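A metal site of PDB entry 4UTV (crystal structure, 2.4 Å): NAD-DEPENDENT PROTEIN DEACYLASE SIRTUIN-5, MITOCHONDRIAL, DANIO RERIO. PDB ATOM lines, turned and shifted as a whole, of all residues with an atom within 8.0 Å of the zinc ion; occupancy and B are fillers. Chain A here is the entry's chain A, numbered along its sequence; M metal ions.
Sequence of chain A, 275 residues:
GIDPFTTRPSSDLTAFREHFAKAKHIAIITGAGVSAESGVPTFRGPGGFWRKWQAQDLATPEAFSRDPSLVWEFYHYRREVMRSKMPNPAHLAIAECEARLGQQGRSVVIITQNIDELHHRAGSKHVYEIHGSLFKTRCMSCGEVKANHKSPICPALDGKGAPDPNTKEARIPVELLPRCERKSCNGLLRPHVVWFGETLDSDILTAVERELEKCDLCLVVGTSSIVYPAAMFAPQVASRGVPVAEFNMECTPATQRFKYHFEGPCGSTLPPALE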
ATOM      1  N   ARG A 138      17.826  15.523  -5.039  1.00  0.00           N
ATOM      2  CA  ARG A 138      17.810  15.202  -6.431  1.00  0.00           C
ATOM      3  C   ARG A 138      18.644  13.929  -6.644  1.00  0.00           C
ATOM      4  O   ARG A 138      19.749  13.814  -6.117  1.00  0.00           O
ATOM      5  CB  ARG A 138      18.393  16.354  -7.241  1.00  0.00           C
ATOM      6  CG  ARG A 138      18.291  16.079  -8.734  1.00  0.00           C
ATOM      7  CD  ARG A 138      18.478  17.286  -9.621  1.00  0.00           C
ATOM      8  NE  ARG A 138      19.833  17.850  -9.734  1.00  0.00           N
ATOM      9  CZ  ARG A 138      20.304  18.961  -9.177  1.00  0.00           C
ATOM     10  NH1 ARG A 138      19.605  19.635  -8.325  1.00  0.00           N
ATOM     11  NH2 ARG A 138      21.531  19.398  -9.467  1.00  0.00           N
ATOM     12  N   CYS A 139      18.078  12.978  -7.391  1.00  0.00           N
ATOM     13  CA  CYS A 139      18.814  11.738  -7.652  1.00  0.00           C
ATOM     14  C   CYS A 139      19.847  11.948  -8.741  1.00  0.00           C
ATOM     15  O   CYS A 139      19.507  12.405  -9.836  1.00  0.00           O
ATOM     16  CB  CYS A 139      17.843  10.635  -8.054  1.00  0.00           C
ATOM     17  SG  CYS A 139      18.584   9.052  -8.413  1.00  0.00           S
ATOM     18  N   MET A 140      21.076  11.573  -8.454  1.00  0.00           N
ATOM     19  CA  MET A 140      22.192  11.700  -9.390  1.00  0.00           C
ATOM     20  C   MET A 140      22.098  10.791 -10.604  1.00  0.00           C
ATOM     21  O   MET A 140      22.752  11.040 -11.640  1.00  0.00           O
ATOM     22  CB  MET A 140      23.511  11.343  -8.733  1.00  0.00           C
ATOM     23  CG  MET A 140      23.927  12.253  -7.598  1.00  0.00           C
ATOM     24  SD  MET A 140      24.389  13.926  -8.084  1.00  0.00           S
ATOM     25  CE  MET A 140      25.912  13.666  -8.991  1.00  0.00           C
ATOM     26  N   SER A 141      21.296   9.755 -10.449  1.00  0.00           N
ATOM     27  CA  SER A 141      21.050   8.735 -11.483  1.00  0.00           C
ATOM     28  C   SER A 141      19.827   8.964 -12.350  1.00  0.00           C
ATOM     29  O   SER A 141      19.992   9.053 -13.534  1.00  0.00           O
ATOM     30  CB  SER A 141      20.936   7.376 -10.812  1.00  0.00           C
ATOM     31  OG  SER A 141      20.990   6.339 -11.725  1.00  0.00           O
ATOM     32  N   CYS A 142      18.612   9.081 -11.789  1.00  0.00           N
ATOM     33  CA  CYS A 142      17.404   9.245 -12.579  1.00  0.00           C
ATOM     34  C   CYS A 142      16.900  10.678 -12.579  1.00  0.00           C
ATOM     35  O   CYS A 142      15.944  10.970 -13.276  1.00  0.00           O
ATOM     36  CB  CYS A 142      16.346   8.348 -12.039  1.00  0.00           C
ATOM     37  SG  CYS A 142      15.643   8.879 -10.455  1.00  0.00           S
ATOM     38  N   GLY A 143      17.491  11.580 -11.787  1.00  0.00           N
ATOM     39  CA  GLY A 143      17.113  13.016 -11.819  1.00  0.00           C
ATOM     40  C   GLY A 143      15.855  13.412 -11.037  1.00  0.00           C
ATOM     41  O   GLY A 143      15.477  14.541 -11.022  1.00  0.00           O
ATOM     42  N   GLU A 144      15.224  12.472 -10.357  1.00  0.00           N
ATOM     43  CA  GLU A 144      14.005  12.743  -9.617  1.00  0.00           C
ATOM     44  C   GLU A 144      14.253  13.709  -8.450  1.00  0.00           C
ATOM     45  O   GLU A 144      15.208  13.546  -7.742  1.00  0.00           O
ATOM     46  CB  GLU A 144      13.448  11.436  -9.031  1.00  0.00           C
ATOM     47  CG  GLU A 144      12.189  11.588  -8.222  1.00  0.00           C
ATOM     48  CD  GLU A 144      11.669  10.222  -7.790  1.00  0.00           C
ATOM     49  OE1 GLU A 144      10.964   9.604  -8.643  1.00  0.00           O
ATOM     50  OE2 GLU A 144      12.059   9.769  -6.677  1.00  0.00           O
ATOM     51  N   VAL A 145      13.376  14.693  -8.302  1.00  0.00           N
ATOM     52  CA  VAL A 145      13.438  15.676  -7.243  1.00  0.00           C
ATOM     53  C   VAL A 145      12.299  15.367  -6.284  1.00  0.00           C
ATOM     54  O   VAL A 145      11.160  15.202  -6.724  1.00  0.00           O
ATOM     55  CB  VAL A 145      13.224  17.070  -7.822  1.00  0.00           C
ATOM     56  CG1 VAL A 145      13.171  18.141  -6.743  1.00  0.00           C
ATOM     57  CG2 VAL A 145      14.348  17.351  -8.798  1.00  0.00           C
ATOM     58  N   ARG A 179      19.925   7.413  -0.440  1.00  0.00           N
ATOM     59  CA  ARG A 179      19.714   6.810  -1.725  1.00  0.00           C
ATOM     60  C   ARG A 179      18.293   7.036  -2.234  1.00  0.00           C
ATOM     61  O   ARG A 179      17.323   7.172  -1.476  1.00  0.00           O
ATOM     62  CB  ARG A 179      19.985   5.329  -1.698  1.00  0.00           C
ATOM     63  CG  ARG A 179      21.330   4.936  -1.100  1.00  0.00           C
ATOM     64  CD  ARG A 179      22.589   5.559  -1.725  1.00  0.00           C
ATOM     65  NE  ARG A 179      22.777   5.140  -3.116  1.00  0.00           N
ATOM     66  CZ  ARG A 179      23.916   5.107  -3.802  1.00  0.00           C
ATOM     67  NH1 ARG A 179      25.072   5.445  -3.261  1.00  0.00           N
ATOM     68  NH2 ARG A 179      23.899   4.733  -5.070  1.00  0.00           N
ATOM     69  N   CYS A 180      18.189   6.988  -3.569  1.00  0.00           N
ATOM     70  CA  CYS A 180      16.896   7.043  -4.267  1.00  0.00           C
ATOM     71  C   CYS A 180      16.031   5.839  -3.964  1.00  0.00           C
ATOM     72  O   CYS A 180      16.484   4.662  -3.958  1.00  0.00           O
ATOM     73  CB  CYS A 180      17.126   7.094  -5.746  1.00  0.00           C
ATOM     74  SG  CYS A 180      15.658   7.411  -6.799  1.00  0.00           S
ATOM     75  N   GLU A 181      14.760   6.113  -3.696  1.00  0.00           N
ATOM     76  CA  GLU A 181      13.882   5.131  -3.099  1.00  0.00           C
ATOM     77  C   GLU A 181      13.111   4.332  -4.102  1.00  0.00           C
ATOM     78  O   GLU A 181      12.398   3.431  -3.720  1.00  0.00           O
ATOM     79  CB  GLU A 181      12.749   5.813  -2.313  1.00  0.00           C
ATOM     80  CG  GLU A 181      13.130   7.032  -1.496  1.00  0.00           C
ATOM     81  CD  GLU A 181      12.621   6.908  -0.083  1.00  0.00           C
ATOM     82  OE1 GLU A 181      13.053   5.918   0.549  1.00  0.00           O
ATOM     83  OE2 GLU A 181      11.809   7.743   0.377  1.00  0.00           O
ATOM     84  N   ARG A 182      13.246   4.638  -5.400  1.00  0.00           N
ATOM     85  CA  ARG A 182      12.727   3.802  -6.487  1.00  0.00           C
ATOM     86  C   ARG A 182      13.612   2.529  -6.589  1.00  0.00           C
ATOM     87  O   ARG A 182      14.802   2.718  -6.811  1.00  0.00           O
ATOM     88  CB  ARG A 182      12.774   4.564  -7.839  1.00  0.00           C
ATOM     89  CG  ARG A 182      12.031   5.916  -7.956  1.00  0.00           C
ATOM     90  CD  ARG A 182      12.252   6.699  -9.310  1.00  0.00           C
ATOM     91  NE  ARG A 182      12.174   5.818 -10.508  1.00  0.00           N
ATOM     92  CZ  ARG A 182      13.136   5.628 -11.429  1.00  0.00           C
ATOM     93  NH1 ARG A 182      14.301   6.264 -11.402  1.00  0.00           N
ATOM     94  NH2 ARG A 182      12.953   4.761 -12.405  1.00  0.00           N
ATOM     95  N   LYS A 183      13.060   1.320  -6.354  1.00  0.00           N
ATOM     96  CA  LYS A 183      13.898   0.119  -6.053  1.00  0.00           C
ATOM     97  C   LYS A 183      14.890  -0.109  -7.188  1.00  0.00           C
ATOM     98  O   LYS A 183      16.093  -0.416  -6.976  1.00  0.00           O
ATOM     99  CB  LYS A 183      13.051  -1.140  -5.817  1.00  0.00           C
ATOM    100  CG  LYS A 183      12.821  -1.514  -4.352  1.00  0.00           C
ATOM    101  CD  LYS A 183      11.633  -2.459  -4.203  1.00  0.00           C
ATOM    102  CE  LYS A 183      10.903  -2.218  -2.885  1.00  0.00           C
ATOM    103  NZ  LYS A 183      10.016  -3.354  -2.514  1.00  0.00           N
ATOM    104  N   SER A 184      14.403   0.105  -8.394  1.00  0.00           N
ATOM    105  CA  SER A 184      15.227  -0.097  -9.581  1.00  0.00           C
ATOM    106  C   SER A 184      16.438   0.844  -9.674  1.00  0.00           C
ATOM    107  O   SER A 184      17.431   0.504 -10.327  1.00  0.00           O
ATOM    108  CB  SER A 184      14.361   0.084 -10.837  1.00  0.00           C
ATOM    109  OG  SER A 184      13.476   1.211 -10.684  1.00  0.00           O
ATOM    110  N   CYS A 185      16.347   2.000  -9.049  1.00  0.00           N
ATOM    111  CA  CYS A 185      17.320   3.053  -9.257  1.00  0.00           C
ATOM    112  C   CYS A 185      18.354   2.975  -8.196  1.00  0.00           C
ATOM    113  O   CYS A 185      19.548   2.717  -8.486  1.00  0.00           O
ATOM    114  CB  CYS A 185      16.655   4.445  -9.301  1.00  0.00           C
ATOM    115  SG  CYS A 185      17.852   5.735  -9.386  1.00  0.00           S
ATOM    116  N   ASN A 186      17.963   3.318  -6.961  1.00  0.00           N
ATOM    117  CA  ASN A 186      18.912   3.418  -5.815  1.00  0.00           C
ATOM    118  C   ASN A 186      20.126   4.362  -5.991  1.00  0.00           C
ATOM    119  O   ASN A 186      21.196   4.156  -5.415  1.00  0.00           O
ATOM    120  CB  ASN A 186      19.380   2.034  -5.382  1.00  0.00           C
ATOM    121  CG  ASN A 186      19.967   1.993  -3.962  1.00  0.00           C
ATOM    122  OD1 ASN A 186      19.296   2.206  -2.978  1.00  0.00           O
ATOM    123  ND2 ASN A 186      21.254   1.689  -3.864  1.00  0.00           N
ATOM    124  N   GLY A 187      19.995   5.392  -6.852  1.00  0.00           N
ATOM    125  CA  GLY A 187      21.050   6.368  -7.092  1.00  0.00           C
ATOM    126  C   GLY A 187      21.407   7.151  -5.821  1.00  0.00           C
ATOM    127  O   GLY A 187      20.613   7.238  -4.860  1.00  0.00           O
ATOM    128  N   LEU A 188      22.621   7.683  -5.786  1.00  0.00           N
ATOM    129  CA  LEU A 188      22.994   8.592  -4.734  1.00  0.00           C
ATOM    130  C   LEU A 188      22.208   9.886  -4.841  1.00  0.00           C
ATOM    131  O   LEU A 188      22.141  10.511  -5.909  1.00  0.00           O
ATOM    132  CB  LEU A 188      24.467   8.916  -4.880  1.00  0.00           C
ATOM    133  CG  LEU A 188      24.983   9.936  -3.913  1.00  0.00           C
ATOM    134  CD1 LEU A 188      24.827   9.444  -2.499  1.00  0.00           C
ATOM    135  CD2 LEU A 188      26.425  10.189  -4.289  1.00  0.00           C
ATOM    136  N   LEU A 189      21.609  10.318  -3.739  1.00  0.00           N
ATOM    137  CA  LEU A 189      20.914  11.588  -3.714  1.00  0.00           C
ATOM    138  C   LEU A 189      21.892  12.681  -3.397  1.00  0.00           C
ATOM    139  O   LEU A 189      22.886  12.463  -2.668  1.00  0.00           O
ATOM    140  CB  LEU A 189      19.805  11.562  -2.686  1.00  0.00           C
ATOM    141  CG  LEU A 189      18.785  10.429  -2.890  1.00  0.00           C
ATOM    142  CD1 LEU A 189      17.682  10.603  -1.892  1.00  0.00           C
ATOM    143  CD2 LEU A 189      18.194  10.452  -4.299  1.00  0.00           C
HETATM  144 ZN    ZN M   1      16.789   7.703  -8.808  1.00  0.00          ZN
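The zinc ion is bound by SG of Cys 139, SG of Cys 185, SG of Cys 180 and SG of Cys 142.
N of Cys 139 is in hydrogen-bond range of O of Glu 144.
The backbone NH of Cys 180 lies within hydrogen-bond range of the backbone carbonyl oxygen of Gly 187 (2.8 Å).
N of Glu 144 sits close to SG of Cys 142 (3.6 Å).
The side-chain sulfur (SG) of Cys 142 lies close to the guanidinium group (NH1) of Arg 182 (3.1 Å).
The side-chain sulfur of Cys 139 lies close to the backbone NH of Ser 141, at 3.5 Å.
The backbone NH of Gly 187 lies close to the side-chain sulfur of Cys 185.
Residues that only touch the zinc ion: Arg 182.
The nearest printed residue that does not touch the zinc ion is Gly 187 (4.4 Å).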
